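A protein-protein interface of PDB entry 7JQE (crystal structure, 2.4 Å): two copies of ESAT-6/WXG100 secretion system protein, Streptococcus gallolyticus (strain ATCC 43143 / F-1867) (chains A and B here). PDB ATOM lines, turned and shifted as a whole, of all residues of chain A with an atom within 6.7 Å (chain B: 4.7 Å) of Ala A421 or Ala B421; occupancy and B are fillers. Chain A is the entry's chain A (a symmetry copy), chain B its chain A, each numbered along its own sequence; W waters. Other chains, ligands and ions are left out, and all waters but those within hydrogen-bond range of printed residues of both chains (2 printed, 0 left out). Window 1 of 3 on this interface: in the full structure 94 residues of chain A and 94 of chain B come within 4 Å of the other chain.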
ATOM      1  N   LYS A 234      14.690  21.989  31.987  1.00  0.00           N
ATOM      2  CA  LYS A 234      15.366  21.291  30.901  1.00  0.00           C
ATOM      3  C   LYS A 234      16.609  22.043  30.453  1.00  0.00           C
ATOM      4  O   LYS A 234      17.647  21.431  30.179  1.00  0.00           O
ATOM      5  CB  LYS A 234      14.403  21.084  29.738  1.00  0.00           C
ATOM      6  CG  LYS A 234      13.121  20.415  30.171  1.00  0.00           C
ATOM      7  CD  LYS A 234      12.199  20.142  29.009  1.00  0.00           C
ATOM      8  CE  LYS A 234      10.947  19.431  29.489  1.00  0.00           C
ATOM      9  NZ  LYS A 234       9.987  19.186  28.381  1.00  0.00           N
ATOM     10  N   LEU A 237      19.374  21.385  32.825  1.00  0.00           N
ATOM     11  CA  LEU A 237      19.971  20.068  32.630  1.00  0.00           C
ATOM     12  C   LEU A 237      20.922  20.065  31.441  1.00  0.00           C
ATOM     13  O   LEU A 237      22.027  19.512  31.524  1.00  0.00           O
ATOM     14  CB  LEU A 237      18.872  19.021  32.449  1.00  0.00           C
ATOM     15  CG  LEU A 237      19.306  17.602  32.071  1.00  0.00           C
ATOM     16  CD1 LEU A 237      20.265  17.028  33.104  1.00  0.00           C
ATOM     17  CD2 LEU A 237      18.096  16.687  31.890  1.00  0.00           C
ATOM     18  N   LEU A 238      20.513  20.673  30.322  1.00  0.00           N
ATOM     19  CA  LEU A 238      21.414  20.783  29.179  1.00  0.00           C
ATOM     20  C   LEU A 238      22.702  21.496  29.564  1.00  0.00           C
ATOM     21  O   LEU A 238      23.764  21.216  28.995  1.00  0.00           O
ATOM     22  CB  LEU A 238      20.728  21.516  28.028  1.00  0.00           C
ATOM     23  CG  LEU A 238      19.441  20.884  27.499  1.00  0.00           C
ATOM     24  CD1 LEU A 238      18.802  21.782  26.444  1.00  0.00           C
ATOM     25  CD2 LEU A 238      19.735  19.522  26.927  1.00  0.00           C
ATOM     26  N   LYS A 415      14.149  21.021  19.870  1.00  0.00           N
ATOM     27  CA  LYS A 415      15.502  20.556  20.158  1.00  0.00           C
ATOM     28  C   LYS A 415      15.748  20.472  21.660  1.00  0.00           C
ATOM     29  O   LYS A 415      16.337  19.499  22.148  1.00  0.00           O
ATOM     30  CB  LYS A 415      16.522  21.476  19.485  1.00  0.00           C
ATOM     31  CG  LYS A 415      16.678  21.175  17.996  1.00  0.00           C
ATOM     32  CD  LYS A 415      17.643  22.121  17.294  1.00  0.00           C
ATOM     33  CE  LYS A 415      16.905  23.334  16.742  1.00  0.00           C
ATOM     34  NZ  LYS A 415      17.766  24.161  15.854  1.00  0.00           N
ATOM     35  N   ILE A 416      15.303  21.480  22.411  1.00  0.00           N
ATOM     36  CA  ILE A 416      15.470  21.457  23.862  1.00  0.00           C
ATOM     37  C   ILE A 416      14.765  20.246  24.457  1.00  0.00           C
ATOM     38  O   ILE A 416      15.303  19.567  25.339  1.00  0.00           O
ATOM     39  CB  ILE A 416      14.957  22.770  24.481  1.00  0.00           C
ATOM     40  CG1 ILE A 416      15.870  23.938  24.104  1.00  0.00           C
ATOM     41  CG2 ILE A 416      14.819  22.645  25.988  1.00  0.00           C
ATOM     42  CD1 ILE A 416      15.179  25.287  24.160  1.00  0.00           C
ATOM     43  N   ASP A 417      13.549  19.956  23.985  1.00  0.00           N
ATOM     44  CA  ASP A 417      12.798  18.839  24.548  1.00  0.00           C
ATOM     45  C   ASP A 417      13.454  17.507  24.210  1.00  0.00           C
ATOM     46  O   ASP A 417      13.593  16.638  25.080  1.00  0.00           O
ATOM     47  CB  ASP A 417      11.352  18.868  24.049  1.00  0.00           C
ATOM     48  CG  ASP A 417      10.495  19.893  24.779  1.00  0.00           C
ATOM     49  OD1 ASP A 417      10.623  20.011  26.017  1.00  0.00           O
ATOM     50  OD2 ASP A 417       9.692  20.579  24.111  1.00  0.00           O
ATOM     51  N   THR A 418      13.870  17.331  22.956  1.00  0.00           N
ATOM     52  CA  THR A 418      14.478  16.076  22.539  1.00  0.00           C
ATOM     53  C   THR A 418      15.759  15.800  23.318  1.00  0.00           C
ATOM     54  O   THR A 418      15.897  14.755  23.960  1.00  0.00           O
ATOM     55  CB  THR A 418      14.752  16.102  21.037  1.00  0.00           C
ATOM     56  OG1 THR A 418      13.505  16.181  20.335  1.00  0.00           O
ATOM     57  CG2 THR A 418      15.500  14.836  20.607  1.00  0.00           C
ATOM     58  N   ALA A 419      16.707  16.738  23.283  1.00  0.00           N
ATOM     59  CA  ALA A 419      17.991  16.511  23.934  1.00  0.00           C
ATOM     60  C   ALA A 419      17.833  16.337  25.441  1.00  0.00           C
ATOM     61  O   ALA A 419      18.487  15.479  26.045  1.00  0.00           O
ATOM     62  CB  ALA A 419      18.946  17.658  23.627  1.00  0.00           C
ATOM     63  N   SER A 420      16.979  17.144  26.069  1.00  0.00           N
ATOM     64  CA  SER A 420      16.781  17.010  27.508  1.00  0.00           C
ATOM     65  C   SER A 420      16.209  15.643  27.860  1.00  0.00           C
ATOM     66  O   SER A 420      16.583  15.051  28.877  1.00  0.00           O
ATOM     67  CB  SER A 420      15.862  18.112  28.026  1.00  0.00           C
ATOM     68  OG  SER A 420      15.787  18.080  29.437  1.00  0.00           O
ATOM     69  N   ALA A 421      15.290  15.133  27.036  1.00  0.00           N
ATOM     70  CA  ALA A 421      14.700  13.827  27.312  1.00  0.00           C
ATOM     71  C   ALA A 421      15.724  12.713  27.136  1.00  0.00           C
ATOM     72  O   ALA A 421      15.735  11.747  27.908  1.00  0.00           O
ATOM     73  CB  ALA A 421      13.490  13.592  26.413  1.00  0.00           C
ATOM     74  N   MET A 422      16.587  12.828  26.131  1.00  0.00           N
ATOM     75  CA  MET A 422      17.660  11.865  25.935  1.00  0.00           C
ATOM     76  C   MET A 422      18.558  11.843  27.163  1.00  0.00           C
ATOM     77  O   MET A 422      18.813  10.788  27.741  1.00  0.00           O
ATOM     78  CB  MET A 422      18.475  12.202  24.692  1.00  0.00           C
ATOM     79  CG  MET A 422      17.735  11.983  23.386  1.00  0.00           C
ATOM     80  SD  MET A 422      18.782  12.582  21.848  1.00  0.00           S
ATOM     81  CE  MET A 422      17.679  11.825  20.427  1.00  0.00           C
ATOM     82  N   ILE A 423      19.024  13.025  27.568  1.00  0.00           N
ATOM     83  CA  ILE A 423      19.873  13.118  28.753  1.00  0.00           C
ATOM     84  C   ILE A 423      19.160  12.526  29.962  1.00  0.00           C
ATOM     85  O   ILE A 423      19.735  11.738  30.721  1.00  0.00           O
ATOM     86  CB  ILE A 423      20.287  14.577  29.001  1.00  0.00           C
ATOM     87  CG1 ILE A 423      21.068  15.112  27.797  1.00  0.00           C
ATOM     88  CG2 ILE A 423      21.114  14.679  30.267  1.00  0.00           C
ATOM     89  CD1 ILE A 423      21.379  16.608  27.870  1.00  0.00           C
ATOM     90  N   GLN A 424      17.893  12.895  30.157  1.00  0.00           N
ATOM     91  CA  GLN A 424      17.132  12.383  31.294  1.00  0.00           C
ATOM     92  C   GLN A 424      17.092  10.857  31.304  1.00  0.00           C
ATOM     93  O   GLN A 424      17.194  10.233  32.368  1.00  0.00           O
ATOM     94  CB  GLN A 424      15.713  12.947  31.256  1.00  0.00           C
ATOM     95  CG  GLN A 424      14.787  12.376  32.305  1.00  0.00           C
ATOM     96  CD  GLN A 424      13.366  12.893  32.165  1.00  0.00           C
ATOM     97  OE1 GLN A 424      12.993  13.447  31.132  1.00  0.00           O
ATOM     98  NE2 GLN A 424      12.563  12.710  33.207  1.00  0.00           N
ATOM     99  N   THR A 425      16.937  10.239  30.131  1.00  0.00           N
ATOM    100  CA  THR A 425      16.732   8.797  30.050  1.00  0.00           C
ATOM    101  C   THR A 425      18.026   8.019  30.240  1.00  0.00           C
ATOM    102  O   THR A 425      17.991   6.859  30.664  1.00  0.00           O
ATOM    103  CB  THR A 425      16.108   8.435  28.702  1.00  0.00           C
ATOM    104  OG1 THR A 425      14.916   9.206  28.503  1.00  0.00           O
ATOM    105  CG2 THR A 425      15.761   6.957  28.651  1.00  0.00           C
ATOM    106  N   LEU A 426      19.166   8.632  29.926  1.00  0.00           N
ATOM    107  CA  LEU A 426      20.456   7.970  30.048  1.00  0.00           C
ATOM    108  C   LEU A 426      21.087   8.163  31.420  1.00  0.00           C
ATOM    109  O   LEU A 426      21.744   7.249  31.927  1.00  0.00           O
ATOM    110  CB  LEU A 426      21.413   8.479  28.967  1.00  0.00           C
ATOM    111  CG  LEU A 426      21.053   8.108  27.525  1.00  0.00           C
ATOM    112  CD1 LEU A 426      21.990   8.785  26.532  1.00  0.00           C
ATOM    113  CD2 LEU A 426      21.075   6.596  27.337  1.00  0.00           C
ATOM    114  N   ASP B 417       7.432  15.394  21.838  1.00  0.00           N
ATOM    115  CA  ASP B 417       8.883  15.375  21.693  1.00  0.00           C
ATOM    116  C   ASP B 417       9.539  14.580  22.815  1.00  0.00           C
ATOM    117  O   ASP B 417      10.437  13.767  22.565  1.00  0.00           O
ATOM    118  CB  ASP B 417       9.432  16.802  21.656  1.00  0.00           C
ATOM    119  CG  ASP B 417       9.244  17.473  20.302  1.00  0.00           C
ATOM    120  OD1 ASP B 417       9.456  16.805  19.266  1.00  0.00           O
ATOM    121  OD2 ASP B 417       8.886  18.669  20.276  1.00  0.00           O
ATOM    122  N   THR B 418       9.099  14.795  24.055  1.00  0.00           N
ATOM    123  CA  THR B 418       9.692  14.102  25.189  1.00  0.00           C
ATOM    124  C   THR B 418       9.510  12.593  25.068  1.00  0.00           C
ATOM    125  O   THR B 418      10.484  11.835  25.090  1.00  0.00           O
ATOM    126  CB  THR B 418       9.083  14.618  26.492  1.00  0.00           C
ATOM    127  OG1 THR B 418       9.430  15.998  26.656  1.00  0.00           O
ATOM    128  CG2 THR B 418       9.612  13.815  27.685  1.00  0.00           C
ATOM    129  N   ALA B 419       8.265  12.140  24.925  1.00  0.00           N
ATOM    130  CA  ALA B 419       8.003  10.705  24.886  1.00  0.00           C
ATOM    131  C   ALA B 419       8.675  10.046  23.686  1.00  0.00           C
ATOM    132  O   ALA B 419       9.229   8.946  23.803  1.00  0.00           O
ATOM    133  CB  ALA B 419       6.502  10.445  24.866  1.00  0.00           C
ATOM    134  N   SER B 420       8.633  10.693  22.522  1.00  0.00           N
ATOM    135  CA  SER B 420       9.273  10.112  21.346  1.00  0.00           C
ATOM    136  C   SER B 420      10.775   9.970  21.551  1.00  0.00           C
ATOM    137  O   SER B 420      11.375   8.981  21.115  1.00  0.00           O
ATOM    138  CB  SER B 420       8.989  10.959  20.111  1.00  0.00           C
ATOM    139  OG  SER B 420       9.476  10.324  18.945  1.00  0.00           O
ATOM    140  N   ALA B 421      11.401  10.954  22.200  1.00  0.00           N
ATOM    141  CA  ALA B 421      12.840  10.882  22.430  1.00  0.00           C
ATOM    142  C   ALA B 421      13.183   9.779  23.424  1.00  0.00           C
ATOM    143  O   ALA B 421      14.194   9.086  23.263  1.00  0.00           O
ATOM    144  CB  ALA B 421      13.365  12.229  22.921  1.00  0.00           C
ATOM    145  N   MET B 422      12.359   9.603  24.452  1.00  0.00           N
ATOM    146  CA  MET B 422      12.547   8.517  25.402  1.00  0.00           C
ATOM    147  C   MET B 422      12.485   7.183  24.674  1.00  0.00           C
ATOM    148  O   MET B 422      13.390   6.358  24.789  1.00  0.00           O
ATOM    149  CB  MET B 422      11.494   8.567  26.504  1.00  0.00           C
ATOM    150  CG  MET B 422      11.651   9.733  27.460  1.00  0.00           C
ATOM    151  SD  MET B 422      10.180   9.821  28.745  1.00  0.00           S
ATOM    152  CE  MET B 422      10.920  11.167  29.948  1.00  0.00           C
ATOM    153  N   ILE B 423      11.413   6.985  23.907  1.00  0.00           N
ATOM    154  CA  ILE B 423      11.270   5.748  23.143  1.00  0.00           C
ATOM    155  C   ILE B 423      12.469   5.551  22.224  1.00  0.00           C
ATOM    156  O   ILE B 423      13.051   4.463  22.157  1.00  0.00           O
ATOM    157  CB  ILE B 423       9.950   5.756  22.355  1.00  0.00           C
ATOM    158  CG1 ILE B 423       8.766   5.878  23.316  1.00  0.00           C
ATOM    159  CG2 ILE B 423       9.834   4.501  21.514  1.00  0.00           C
ATOM    160  CD1 ILE B 423       7.414   6.067  22.622  1.00  0.00           C
ATOM    161  N   GLN B 424      12.859   6.605  21.505  1.00  0.00           N
ATOM    162  CA  GLN B 424      13.996   6.508  20.593  1.00  0.00           C
ATOM    163  C   GLN B 424      15.260   6.047  21.314  1.00  0.00           C
ATOM    164  O   GLN B 424      16.035   5.248  20.776  1.00  0.00           O
ATOM    165  CB  GLN B 424      14.233   7.860  19.925  1.00  0.00           C
ATOM    166  CG  GLN B 424      15.473   7.921  19.064  1.00  0.00           C
ATOM    167  CD  GLN B 424      15.720   9.310  18.501  1.00  0.00           C
ATOM    168  OE1 GLN B 424      15.144  10.292  18.969  1.00  0.00           O
ATOM    169  NE2 GLN B 424      16.581   9.397  17.495  1.00  0.00           N
ATOM    170  N   THR B 425      15.488   6.546  22.531  1.00  0.00           N
ATOM    171  CA  THR B 425      16.739   6.292  23.237  1.00  0.00           C
ATOM    172  C   THR B 425      16.783   4.898  23.847  1.00  0.00           C
ATOM    173  O   THR B 425      17.871   4.349  24.054  1.00  0.00           O
ATOM    174  CB  THR B 425      16.941   7.339  24.333  1.00  0.00           C
ATOM    175  OG1 THR B 425      16.847   8.651  23.765  1.00  0.00           O
ATOM    176  CG2 THR B 425      18.300   7.174  24.990  1.00  0.00           C
HETATM  177  O   HOH W   1      11.915  16.557  27.451  1.00  0.00           O
HETATM  178  O   HOH W   2      12.051  13.953  20.156  1.00  0.00           O
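OG1 of Thr B425 is in hydrogen-bond range of O of Ala B421, at 2.7 Å.
The side-chain amino group (NZ) of Lys A234 is in salt-bridge range of the side-chain carboxylate (OD1) of Asp A417, 2.6 Å away.
The backbone carbonyl oxygen of Ala A421 is in hydrogen-bond range of the side-chain hydroxyl of Thr A425, at 2.7 Å.
Water W2 lies within hydrogen-bond range of OG1 of Thr A418 and O of Asp B417.
Water W1 lies within hydrogen-bond range of the side-chain hydroxyl of Thr B418 (2.7 Å), the backbone carbonyl oxygen of Asp A417 (2.9 Å) and the side-chain amino group of Lys A234 (3.4 Å).
Of the 9 printed residues of chain B, 6 touch a printed residue of chain A.
Along chain B the printed residues that touch a printed residue of chain A span positions 417 to 425.
Of the 15 printed residues of chain A, 8 touch a printed residue of chain B.
Printed residues of chain A that touch a printed residue of chain B: Lys A234, Asp A417, Thr A418, Ala A421, Met A422, Gln A424, Thr A425 and Leu A426.
Among the printed residues, no Asp or Glu carboxylate lies within 4 Å of a Lys or Arg side-chain nitrogen of the other chain.
Among the printed residues, pairs that only touch across the chains: Lys A234 with Thr B418 (3.7 Å), Asp A417 with Asp B417 (3.7 Å), Thr A418 with Ala B421 (3.7 Å), Ala A421 with Thr B418 (3.7 Å), Ala A421 with Ala B421 (3.8 Å), Met A422 with Gln B424 (3.3 Å), Met A422 with Thr B425 (3.5 Å), Gln A424 with Met B422 (3.3 Å), Thr A425 with Met B422 (3.5 Å) and Leu A426 with Thr B425 (3.7 Å).
Ala A421 touches just these residues of chain B: Thr B418 and Ala B421.
Of chain A, only Thr A418 and Ala A421 come within 4 Å of Ala B421.
Printed residues of chain B within 4 Å of Met A422: Gln B424 and Thr B425.
Of the printed residues of chain B, Thr A425 touches Met B422 (3.5 Å).
Of the printed residues of chain A, Thr B425 touches Met A422 and Leu A426.
Ser B420 touches none of the printed residues of chain A.
Ile A416 touches none of the printed residues of chain B.
The nearest residue of chain B that does not touch Ala A421 is Met B422 (4.4 Å).
The nearest residue of chain A that does not touch Ala B421 is Met A422 (4.4 Å).
The nearest printed residue of chain A that does not touch Thr B418 is Asp A417 (4.2 Å).
Thr A418 touches Ala B421, and with the chains exchanged Ala A421 touches Thr B418.
Ala A421 touches its own counterpart, Ala B421.
Met A422 touches Gln B424, and with the chains exchanged Gln A424 touches Met B422.
Met A422 touches Thr B425, and with the chains exchanged Thr A425 touches Met B422.
Positions printed for both chains: 417, 418, 419, 420, 421, 422, 423, 424 and 425.
Of the 10 pairs that touch across the chains among the printed residues, 8 have their exchanged pair printed and touching as well.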
